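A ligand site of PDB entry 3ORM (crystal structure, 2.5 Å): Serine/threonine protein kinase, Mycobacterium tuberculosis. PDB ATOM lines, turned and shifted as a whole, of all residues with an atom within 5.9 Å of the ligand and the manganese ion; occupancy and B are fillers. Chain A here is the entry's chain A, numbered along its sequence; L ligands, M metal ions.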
ATOM      1  N   LEU A  20     -12.411  11.713  16.596  1.00  0.00           N
ATOM      2  CA  LEU A  20     -13.187  10.591  16.071  1.00  0.00           C
ATOM      3  C   LEU A  20     -14.093  11.051  14.945  1.00  0.00           C
ATOM      4  O   LEU A  20     -14.300  10.326  13.971  1.00  0.00           O
ATOM      5  CB  LEU A  20     -14.002   9.945  17.187  1.00  0.00           C
ATOM      6  CG  LEU A  20     -13.239   8.953  18.070  1.00  0.00           C
ATOM      7  CD1 LEU A  20     -14.094   8.502  19.236  1.00  0.00           C
ATOM      8  CD2 LEU A  20     -12.775   7.764  17.248  1.00  0.00           C
ATOM      9  N   GLY A  21     -14.646  12.250  15.074  1.00  0.00           N
ATOM     10  CA  GLY A  21     -15.560  12.761  14.063  1.00  0.00           C
ATOM     11  C   GLY A  21     -16.034  14.172  14.317  1.00  0.00           C
ATOM     12  O   GLY A  21     -15.837  14.722  15.400  1.00  0.00           O
ATOM     13  N   PHE A  22     -16.676  14.759  13.308  1.00  0.00           N
ATOM     14  CA  PHE A  22     -17.183  16.114  13.407  1.00  0.00           C
ATOM     15  C   PHE A  22     -18.673  16.155  13.129  1.00  0.00           C
ATOM     16  O   PHE A  22     -19.142  15.569  12.157  1.00  0.00           O
ATOM     17  CB  PHE A  22     -16.464  17.035  12.431  1.00  0.00           C
ATOM     18  CG  PHE A  22     -15.000  17.194  12.696  1.00  0.00           C
ATOM     19  CD1 PHE A  22     -14.552  18.088  13.657  1.00  0.00           C
ATOM     20  CD2 PHE A  22     -14.068  16.447  11.989  1.00  0.00           C
ATOM     21  CE1 PHE A  22     -13.196  18.231  13.918  1.00  0.00           C
ATOM     22  CE2 PHE A  22     -12.715  16.588  12.237  1.00  0.00           C
ATOM     23  CZ  PHE A  22     -12.281  17.479  13.194  1.00  0.00           C
ATOM     24  N   GLY A  23     -19.407  16.840  14.000  1.00  0.00           N
ATOM     25  CA  GLY A  23     -20.832  17.012  13.822  1.00  0.00           C
ATOM     26  C   GLY A  23     -21.144  18.478  13.595  1.00  0.00           C
ATOM     27  O   GLY A  23     -20.272  19.327  13.758  1.00  0.00           O
ATOM     28  N   GLY A  24     -22.383  18.769  13.210  1.00  0.00           N
ATOM     29  CA  GLY A  24     -22.799  20.136  12.987  1.00  0.00           C
ATOM     30  C   GLY A  24     -22.778  20.970  14.261  1.00  0.00           C
ATOM     31  O   GLY A  24     -22.965  22.181  14.217  1.00  0.00           O
ATOM     32  N   MET A  25     -22.541  20.331  15.391  1.00  0.00           N
ATOM     33  CA  MET A  25     -22.624  21.026  16.673  1.00  0.00           C
ATOM     34  C   MET A  25     -21.399  20.818  17.563  1.00  0.00           C
ATOM     35  O   MET A  25     -21.225  21.548  18.545  1.00  0.00           O
ATOM     36  CB  MET A  25     -23.852  20.542  17.439  1.00  0.00           C
ATOM     37  CG  MET A  25     -25.019  21.515  17.421  1.00  0.00           C
ATOM     38  SD  MET A  25     -26.262  21.101  18.649  1.00  0.00           S
ATOM     39  CE  MET A  25     -25.296  21.196  20.151  1.00  0.00           C
ATOM     40  N   SER A  26     -20.561  19.849  17.239  1.00  0.00           N
ATOM     41  CA  SER A  26     -19.543  19.416  18.183  1.00  0.00           C
ATOM     42  C   SER A  26     -18.348  18.729  17.564  1.00  0.00           C
ATOM     43  O   SER A  26     -18.341  18.355  16.396  1.00  0.00           O
ATOM     44  CB  SER A  26     -20.191  18.452  19.180  1.00  0.00           C
ATOM     45  OG  SER A  26     -20.720  17.328  18.496  1.00  0.00           O
ATOM     46  N   VAL A  28     -16.010  15.390  18.419  1.00  0.00           N
ATOM     47  CA  VAL A  28     -15.987  14.196  19.255  1.00  0.00           C
ATOM     48  C   VAL A  28     -14.598  13.585  19.283  1.00  0.00           C
ATOM     49  O   VAL A  28     -14.058  13.200  18.258  1.00  0.00           O
ATOM     50  CB  VAL A  28     -16.974  13.141  18.740  1.00  0.00           C
ATOM     51  CG1 VAL A  28     -17.006  11.941  19.689  1.00  0.00           C
ATOM     52  CG2 VAL A  28     -18.370  13.746  18.597  1.00  0.00           C
ATOM     53  N   ALA A  41     -15.848   8.170  24.292  1.00  0.00           N
ATOM     54  CA  ALA A  41     -16.021   9.243  23.327  1.00  0.00           C
ATOM     55  C   ALA A  41     -16.438  10.493  24.085  1.00  0.00           C
ATOM     56  O   ALA A  41     -17.453  10.489  24.784  1.00  0.00           O
ATOM     57  CB  ALA A  41     -17.050   8.860  22.295  1.00  0.00           C
ATOM     58  N   LYS A  43     -17.729  14.212  23.688  1.00  0.00           N
ATOM     59  CA  LYS A  43     -18.388  15.149  22.795  1.00  0.00           C
ATOM     60  C   LYS A  43     -18.225  16.555  23.347  1.00  0.00           C
ATOM     61  O   LYS A  43     -18.731  16.860  24.430  1.00  0.00           O
ATOM     62  CB  LYS A  43     -19.864  14.799  22.702  1.00  0.00           C
ATOM     63  CG  LYS A  43     -20.573  15.418  21.539  1.00  0.00           C
ATOM     64  CD  LYS A  43     -21.967  14.820  21.425  1.00  0.00           C
ATOM     65  CE  LYS A  43     -22.858  15.641  20.523  1.00  0.00           C
ATOM     66  NZ  LYS A  43     -24.079  14.875  20.185  1.00  0.00           N
ATOM     67  N   ARG A  58     -29.429  23.468  24.221  1.00  0.00           N
ATOM     68  CA  ARG A  58     -29.709  22.274  23.428  1.00  0.00           C
ATOM     69  C   ARG A  58     -28.756  21.174  23.869  1.00  0.00           C
ATOM     70  O   ARG A  58     -29.173  20.080  24.274  1.00  0.00           O
ATOM     71  CB  ARG A  58     -29.529  22.573  21.933  1.00  0.00           C
ATOM     72  CG  ARG A  58     -30.251  21.585  20.994  1.00  0.00           C
ATOM     73  CD  ARG A  58     -29.539  21.442  19.644  1.00  0.00           C
ATOM     74  NE  ARG A  58     -30.460  21.415  18.514  1.00  0.00           N
ATOM     75  CZ  ARG A  58     -30.454  20.510  17.535  1.00  0.00           C
ATOM     76  NH1 ARG A  58     -29.560  19.531  17.514  1.00  0.00           N
ATOM     77  NH2 ARG A  58     -31.348  20.596  16.555  1.00  0.00           N
ATOM     78  N   GLU A  62     -30.039  17.629  25.586  1.00  0.00           N
ATOM     79  CA  GLU A  62     -29.794  16.358  24.917  1.00  0.00           C
ATOM     80  C   GLU A  62     -29.064  15.397  25.844  1.00  0.00           C
ATOM     81  O   GLU A  62     -29.347  14.192  25.889  1.00  0.00           O
ATOM     82  CB  GLU A  62     -28.998  16.597  23.636  1.00  0.00           C
ATOM     83  CG  GLU A  62     -29.864  17.100  22.493  1.00  0.00           C
ATOM     84  CD  GLU A  62     -29.047  17.656  21.328  1.00  0.00           C
ATOM     85  OE1 GLU A  62     -27.829  17.858  21.489  1.00  0.00           O
ATOM     86  OE2 GLU A  62     -29.647  17.888  20.255  1.00  0.00           O
ATOM     87  N   VAL A  75     -26.084   4.010  22.361  1.00  0.00           N
ATOM     88  CA  VAL A  75     -24.915   4.595  22.992  1.00  0.00           C
ATOM     89  C   VAL A  75     -25.243   5.182  24.370  1.00  0.00           C
ATOM     90  O   VAL A  75     -26.043   6.109  24.480  1.00  0.00           O
ATOM     91  CB  VAL A  75     -24.345   5.724  22.103  1.00  0.00           C
ATOM     92  CG1 VAL A  75     -23.215   6.469  22.809  1.00  0.00           C
ATOM     93  CG2 VAL A  75     -23.869   5.148  20.777  1.00  0.00           C
ATOM     94  N   MET A  95     -19.240   9.601  26.736  1.00  0.00           N
ATOM     95  CA  MET A  95     -20.068   8.452  26.392  1.00  0.00           C
ATOM     96  C   MET A  95     -19.298   7.187  26.008  1.00  0.00           C
ATOM     97  O   MET A  95     -18.091   7.203  25.741  1.00  0.00           O
ATOM     98  CB  MET A  95     -21.048   8.784  25.263  1.00  0.00           C
ATOM     99  CG  MET A  95     -20.464   9.604  24.137  1.00  0.00           C
ATOM    100  SD  MET A  95     -21.688  10.038  22.875  1.00  0.00           S
ATOM    101  CE  MET A  95     -20.764  11.253  21.950  1.00  0.00           C
ATOM    102  N   GLU A  96     -20.053   6.091  25.992  1.00  0.00           N
ATOM    103  CA  GLU A  96     -19.569   4.836  25.460  1.00  0.00           C
ATOM    104  C   GLU A  96     -18.973   5.040  24.085  1.00  0.00           C
ATOM    105  O   GLU A  96     -19.573   5.683  23.221  1.00  0.00           O
ATOM    106  CB  GLU A  96     -20.707   3.825  25.346  1.00  0.00           C
ATOM    107  CG  GLU A  96     -20.413   2.744  24.326  1.00  0.00           C
ATOM    108  CD  GLU A  96     -21.584   1.834  24.099  1.00  0.00           C
ATOM    109  OE1 GLU A  96     -21.389   0.840  23.379  1.00  0.00           O
ATOM    110  OE2 GLU A  96     -22.684   2.106  24.616  1.00  0.00           O
ATOM    111  N   TYR A  97     -17.792   4.474  23.879  1.00  0.00           N
ATOM    112  CA  TYR A  97     -17.072   4.596  22.624  1.00  0.00           C
ATOM    113  C   TYR A  97     -17.412   3.442  21.674  1.00  0.00           C
ATOM    114  O   TYR A  97     -17.304   2.269  22.011  1.00  0.00           O
ATOM    115  CB  TYR A  97     -15.579   4.627  22.916  1.00  0.00           C
ATOM    116  CG  TYR A  97     -14.675   4.267  21.748  1.00  0.00           C
ATOM    117  CD1 TYR A  97     -14.645   5.040  20.615  1.00  0.00           C
ATOM    118  CD2 TYR A  97     -13.846   3.165  21.803  1.00  0.00           C
ATOM    119  CE1 TYR A  97     -13.831   4.713  19.543  1.00  0.00           C
ATOM    120  CE2 TYR A  97     -13.028   2.839  20.744  1.00  0.00           C
ATOM    121  CZ  TYR A  97     -13.017   3.620  19.624  1.00  0.00           C
ATOM    122  OH  TYR A  97     -12.207   3.291  18.538  1.00  0.00           O
ATOM    123  N   VAL A  98     -17.858   3.815  20.484  1.00  0.00           N
ATOM    124  CA  VAL A  98     -18.099   2.848  19.413  1.00  0.00           C
ATOM    125  C   VAL A  98     -16.909   2.907  18.458  1.00  0.00           C
ATOM    126  O   VAL A  98     -16.590   3.975  17.929  1.00  0.00           O
ATOM    127  CB  VAL A  98     -19.397   3.170  18.657  1.00  0.00           C
ATOM    128  CG1 VAL A  98     -19.595   2.202  17.500  1.00  0.00           C
ATOM    129  CG2 VAL A  98     -20.588   3.122  19.604  1.00  0.00           C
ATOM    130  N   ASP A  99     -16.219   1.788  18.274  1.00  0.00           N
ATOM    131  CA  ASP A  99     -15.152   1.726  17.294  1.00  0.00           C
ATOM    132  C   ASP A  99     -15.724   1.152  16.025  1.00  0.00           C
ATOM    133  O   ASP A  99     -15.856  -0.064  15.880  1.00  0.00           O
ATOM    134  CB  ASP A  99     -13.990   0.861  17.790  1.00  0.00           C
ATOM    135  CG  ASP A  99     -12.843   0.791  16.795  1.00  0.00           C
ATOM    136  OD1 ASP A  99     -12.860   1.560  15.802  1.00  0.00           O
ATOM    137  OD2 ASP A  99     -11.915  -0.023  17.006  1.00  0.00           O
ATOM    138  N   GLY A 100     -16.096   2.031  15.108  1.00  0.00           N
ATOM    139  CA  GLY A 100     -16.782   1.625  13.905  1.00  0.00           C
ATOM    140  C   GLY A 100     -17.125   2.827  13.064  1.00  0.00           C
ATOM    141  O   GLY A 100     -16.355   3.781  12.994  1.00  0.00           O
ATOM    142  N   THR A 102     -20.448   5.309  10.941  1.00  0.00           N
ATOM    143  CA  THR A 102     -21.865   5.642  10.766  1.00  0.00           C
ATOM    144  C   THR A 102     -22.387   5.082   9.429  1.00  0.00           C
ATOM    145  O   THR A 102     -21.603   4.693   8.572  1.00  0.00           O
ATOM    146  CB  THR A 102     -22.123   7.180  10.833  1.00  0.00           C
ATOM    147  OG1 THR A 102     -21.570   7.809   9.677  1.00  0.00           O
ATOM    148  CG2 THR A 102     -21.498   7.788  12.098  1.00  0.00           C
ATOM    149  N   ARG A 104     -23.963   6.692   7.199  1.00  0.00           N
ATOM    150  CA  ARG A 104     -23.594   7.679   6.190  1.00  0.00           C
ATOM    151  C   ARG A 104     -22.240   7.351   5.569  1.00  0.00           C
ATOM    152  O   ARG A 104     -22.088   7.312   4.347  1.00  0.00           O
ATOM    153  CB  ARG A 104     -23.485   9.059   6.805  1.00  0.00           C
ATOM    154  CG  ARG A 104     -22.839  10.060   5.871  1.00  0.00           C
ATOM    155  CD  ARG A 104     -22.932  11.436   6.433  1.00  0.00           C
ATOM    156  NE  ARG A 104     -22.200  11.571   7.695  1.00  0.00           N
ATOM    157  CZ  ARG A 104     -22.236  12.665   8.433  1.00  0.00           C
ATOM    158  NH1 ARG A 104     -22.981  13.682   8.045  1.00  0.00           N
ATOM    159  NH2 ARG A 104     -21.565  12.740   9.571  1.00  0.00           N
ATOM    160  N   ASP A 105     -21.266   7.124   6.437  1.00  0.00           N
ATOM    161  CA  ASP A 105     -19.923   6.755   6.024  1.00  0.00           C
ATOM    162  C   ASP A 105     -19.971   5.475   5.218  1.00  0.00           C
ATOM    163  O   ASP A 105     -19.395   5.397   4.129  1.00  0.00           O
ATOM    164  CB  ASP A 105     -19.028   6.574   7.242  1.00  0.00           C
ATOM    165  CG  ASP A 105     -18.727   7.887   7.957  1.00  0.00           C
ATOM    166  OD1 ASP A 105     -18.595   8.926   7.270  1.00  0.00           O
ATOM    167  OD2 ASP A 105     -18.598   7.875   9.201  1.00  0.00           O
ATOM    168  N   ASP A 141     -34.440  12.671  15.200  1.00  0.00           N
ATOM    169  CA  ASP A 141     -33.331  13.042  14.325  1.00  0.00           C
ATOM    170  C   ASP A 141     -32.674  11.782  13.788  1.00  0.00           C
ATOM    171  O   ASP A 141     -31.469  11.740  13.550  1.00  0.00           O
ATOM    172  CB  ASP A 141     -32.307  13.891  15.095  1.00  0.00           C
ATOM    173  CG  ASP A 141     -31.271  14.552  14.188  1.00  0.00           C
ATOM    174  OD1 ASP A 141     -31.594  14.852  13.022  1.00  0.00           O
ATOM    175  OD2 ASP A 141     -30.130  14.770  14.658  1.00  0.00           O
ATOM    176  N   LYS A 143     -31.205   9.520  11.356  1.00  0.00           N
ATOM    177  CA  LYS A 143     -30.596   9.753  10.054  1.00  0.00           C
ATOM    178  C   LYS A 143     -29.343   8.894   9.947  1.00  0.00           C
ATOM    179  O   LYS A 143     -28.862   8.367  10.952  1.00  0.00           O
ATOM    180  CB  LYS A 143     -30.274  11.234   9.902  1.00  0.00           C
ATOM    181  CG  LYS A 143     -29.421  11.808  11.024  1.00  0.00           C
ATOM    182  CD  LYS A 143     -29.037  13.254  10.740  1.00  0.00           C
ATOM    183  CE  LYS A 143     -28.071  13.808  11.779  1.00  0.00           C
ATOM    184  NZ  LYS A 143     -27.597  15.163  11.390  1.00  0.00           N
ATOM    185  N   ALA A 145     -26.265   9.384   9.751  1.00  0.00           N
ATOM    186  CA  ALA A 145     -25.100   9.792  10.535  1.00  0.00           C
ATOM    187  C   ALA A 145     -25.247   9.488  12.021  1.00  0.00           C
ATOM    188  O   ALA A 145     -24.261   9.453  12.754  1.00  0.00           O
ATOM    189  CB  ALA A 145     -24.830  11.266  10.354  1.00  0.00           C
ATOM    190  N   ASN A 146     -26.484   9.296  12.456  1.00  0.00           N
ATOM    191  CA  ASN A 146     -26.771   9.047  13.858  1.00  0.00           C
ATOM    192  C   ASN A 146     -26.871   7.564  14.206  1.00  0.00           C
ATOM    193  O   ASN A 146     -27.239   7.215  15.324  1.00  0.00           O
ATOM    194  CB  ASN A 146     -28.032   9.777  14.277  1.00  0.00           C
ATOM    195  CG  ASN A 146     -27.767  11.216  14.678  1.00  0.00           C
ATOM    196  OD1 ASN A 146     -26.610  11.622  14.784  1.00  0.00           O
ATOM    197  ND2 ASN A 146     -28.819  11.982  14.907  1.00  0.00           N
ATOM    198  N   MET A 148     -24.497   4.036  14.094  1.00  0.00           N
ATOM    199  CA  MET A 148     -23.173   3.484  13.897  1.00  0.00           C
ATOM    200  C   MET A 148     -23.205   1.969  13.866  1.00  0.00           C
ATOM    201  O   MET A 148     -24.116   1.349  14.429  1.00  0.00           O
ATOM    202  CB  MET A 148     -22.210   3.962  14.990  1.00  0.00           C
ATOM    203  CG  MET A 148     -21.720   5.393  14.773  1.00  0.00           C
ATOM    204  SD  MET A 148     -20.415   5.899  15.905  1.00  0.00           S
ATOM    205  CE  MET A 148     -18.969   5.337  15.024  1.00  0.00           C
ATOM    206  N   MET A 158     -27.597   6.846  18.253  1.00  0.00           N
ATOM    207  CA  MET A 158     -27.025   7.897  19.073  1.00  0.00           C
ATOM    208  C   MET A 158     -27.592   9.268  18.759  1.00  0.00           C
ATOM    209  O   MET A 158     -28.401   9.440  17.842  1.00  0.00           O
ATOM    210  CB  MET A 158     -25.505   7.935  18.876  1.00  0.00           C
ATOM    211  CG  MET A 158     -25.076   8.417  17.505  1.00  0.00           C
ATOM    212  SD  MET A 158     -23.294   8.356  17.265  1.00  0.00           S
ATOM    213  CE  MET A 158     -23.160   9.028  15.611  1.00  0.00           C
ATOM    214  N   ASP A 159     -27.144  10.261  19.532  1.00  0.00           N
ATOM    215  CA  ASP A 159     -27.504  11.652  19.326  1.00  0.00           C
ATOM    216  C   ASP A 159     -29.019  11.839  19.387  1.00  0.00           C
ATOM    217  O   ASP A 159     -29.619  12.446  18.497  1.00  0.00           O
ATOM    218  CB  ASP A 159     -26.940  12.152  17.995  1.00  0.00           C
ATOM    219  CG  ASP A 159     -26.944  13.666  17.896  1.00  0.00           C
ATOM    220  OD1 ASP A 159     -26.839  14.331  18.950  1.00  0.00           O
ATOM    221  OD2 ASP A 159     -27.019  14.185  16.762  1.00  0.00           O
ATOM    222  N   THR A 182     -29.477  17.855   9.850  1.00  0.00           N
ATOM    223  CA  THR A 182     -30.063  18.086   8.538  1.00  0.00           C
ATOM    224  C   THR A 182     -31.583  18.250   8.639  1.00  0.00           C
ATOM    225  O   THR A 182     -32.153  18.535   9.697  1.00  0.00           O
ATOM    226  CB  THR A 182     -29.707  16.920   7.552  1.00  0.00           C
ATOM    227  OG1 THR A 182     -28.375  16.483   7.807  1.00  0.00           O
ATOM    228  CG2 THR A 182     -29.823  17.344   6.055  1.00  0.00           C
HETATM  229  P1  LIG L   1     -25.298  16.836  14.362  1.00  0.00           P
HETATM  230  S1  LIG L   1     -26.214  18.034  15.697  1.00  0.00           S
HETATM  231  O1  LIG L   1     -25.092  17.647  13.116  1.00  0.00           O
HETATM  232  O2  LIG L   1     -26.200  15.613  14.054  1.00  0.00           O
HETATM  233  P2  LIG L   1     -23.536  16.364  16.427  1.00  0.00           P
HETATM  234  O3  LIG L   1     -22.972  17.775  16.760  1.00  0.00           O
HETATM  235  O4  LIG L   1     -24.747  16.107  17.282  1.00  0.00           O
HETATM  236  O5  LIG L   1     -23.906  16.325  14.903  1.00  0.00           O
HETATM  237  P3  LIG L   1     -22.730  13.710  16.792  1.00  0.00           P
HETATM  238  O6  LIG L   1     -23.289  13.266  18.175  1.00  0.00           O
HETATM  239  O7  LIG L   1     -23.679  13.241  15.724  1.00  0.00           O
HETATM  240  O8  LIG L   1     -22.446  15.269  16.724  1.00  0.00           O
HETATM  241  O9  LIG L   1     -21.352  13.037  16.548  1.00  0.00           O
HETATM  242  C1  LIG L   1     -20.649  13.391  15.392  1.00  0.00           C
HETATM  243  C2  LIG L   1     -19.575  12.398  15.010  1.00  0.00           C
HETATM  244  O10 LIG L   1     -18.447  12.038  15.855  1.00  0.00           O
HETATM  245  C3  LIG L   1     -19.717  11.357  13.903  1.00  0.00           C
HETATM  246  O11 LIG L   1     -20.813  11.181  13.083  1.00  0.00           O
HETATM  247  C4  LIG L   1     -18.675  10.313  14.261  1.00  0.00           C
HETATM  248  O12 LIG L   1     -17.909   9.609  13.338  1.00  0.00           O
HETATM  249  C5  LIG L   1     -18.337  10.585  15.732  1.00  0.00           C
HETATM  250  N1  LIG L   1     -18.911   9.958  16.917  1.00  0.00           N
HETATM  251  C6  LIG L   1     -19.975  10.415  17.574  1.00  0.00           C
HETATM  252  N2  LIG L   1     -20.241   9.566  18.642  1.00  0.00           N
HETATM  253  C7  LIG L   1     -19.293   8.580  18.621  1.00  0.00           C
HETATM  254  C8  LIG L   1     -19.092   7.501  19.446  1.00  0.00           C
HETATM  255  N3  LIG L   1     -19.980   7.275  20.538  1.00  0.00           N
HETATM  256  N4  LIG L   1     -18.078   6.674  19.219  1.00  0.00           N
HETATM  257  C9  LIG L   1     -17.251   6.888  18.175  1.00  0.00           C
HETATM  258  N5  LIG L   1     -17.448   7.950  17.351  1.00  0.00           N
HETATM  259  C10 LIG L   1     -18.469   8.800  17.585  1.00  0.00           C
HETATM  260 MN    MN M   1     -26.828  16.446  17.667  1.00  0.00          MN
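An oxygen (O6) of the ligand lies within salt-bridge range of the side-chain amino group (NZ) of Lys 43. The backbone NH (N) of Ser 26 sits at hydrogen-bond distance from an oxygen (O3) of the ligand. The side-chain hydroxyl (OG) of Ser 26 lies within hydrogen-bond range of an oxygen (O3) of the ligand (2.9 Å). The backbone NH (N) of Met 25 sits at hydrogen-bond distance from an oxygen (O3) of the ligand, 2.9 Å away. N of Gly 24 lies within hydrogen-bond range of O1 of the ligand, at 2.9 Å. The backbone NH of Val 98 sits at hydrogen-bond distance from a nitrogen (N4) of the ligand (3.1 Å). An oxygen (O2) of the ligand is in hydrogen-bond range of the side-chain amino group (NZ) of Lys 143, at 3.0 Å. The backbone carbonyl oxygen (O) of Glu 96 is in hydrogen-bond range of a nitrogen (N3) of the ligand, at 3.1 Å. The side-chain amide oxygen (OD1) of Asn 146 lies close to an oxygen (O7) of the ligand (3.5 Å).
NZ of Lys 43 sits close to OD1 of Asp 159 (3.1 Å). The side-chain carboxylate (OD2) of Asp 159 lies close to the side-chain amide oxygen (OD1) of Asn 146. The backbone carbonyl oxygen (O) of Gly 21 is in hydrogen-bond range of the backbone NH (N) of Val 28 (3.1 Å). O of Val 28 lies within hydrogen-bond range of N of Leu 20 (2.8 Å). O of Asn 146 is in hydrogen-bond range of N of Met 158, 3.0 Å away. The side-chain amide nitrogen (ND2) of Asn 146 lies within hydrogen-bond range of the backbone carbonyl oxygen (O) of Asp 141 (3.0 Å). OG1 of Thr 102 lies within hydrogen-bond range of OD2 of Asp 105. N of Met 95 is in hydrogen-bond range of O of Ala 41 (2.8 Å).
N2 of the ligand lies close to SD of Met 158, at 3.6 Å. CD1 of Leu 20 touches C9 of the ligand (3.7 Å). CA of Gly 21 touches O10 of the ligand, 3.5 Å away. Gly 23 touches the ligand (CA to O5, 3.3 Å). Val 28 touches the ligand. CB of Ala 41 touches C8 of the ligand, 3.8 Å away. Met 95 touches the ligand (CE to N2, 3.7 Å). Thr 102 touches the ligand. Arg 104 touches the ligand. Ala 145 touches the ligand (O to O11, 3.9 Å). Met 148 touches the ligand (CE to N5, 3.8 Å). Hydrophobic or aromatic side chains that line the ligand: Leu 20, Met 25, Val 28, Ala 41, Met 95, Val 98, Met 148 and Met 158. The nearest printed residue that does not touch the ligand is Tyr 97 (4.02 Å).
One residue has an atom within 4 Å of the manganese ion: Asp 159.
The manganese ion is bound by an oxygen (O4) of the ligand (2.1 Å), the side-chain carboxylate (OD2) of Asp 159 (2.4 Å), the side-chain carboxylate (OD1) of Asp 159 (2.5 Å) and a sulfur (S1) of the ligand (2.6 Å). The manganese ion has four donor atoms within binding distance.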
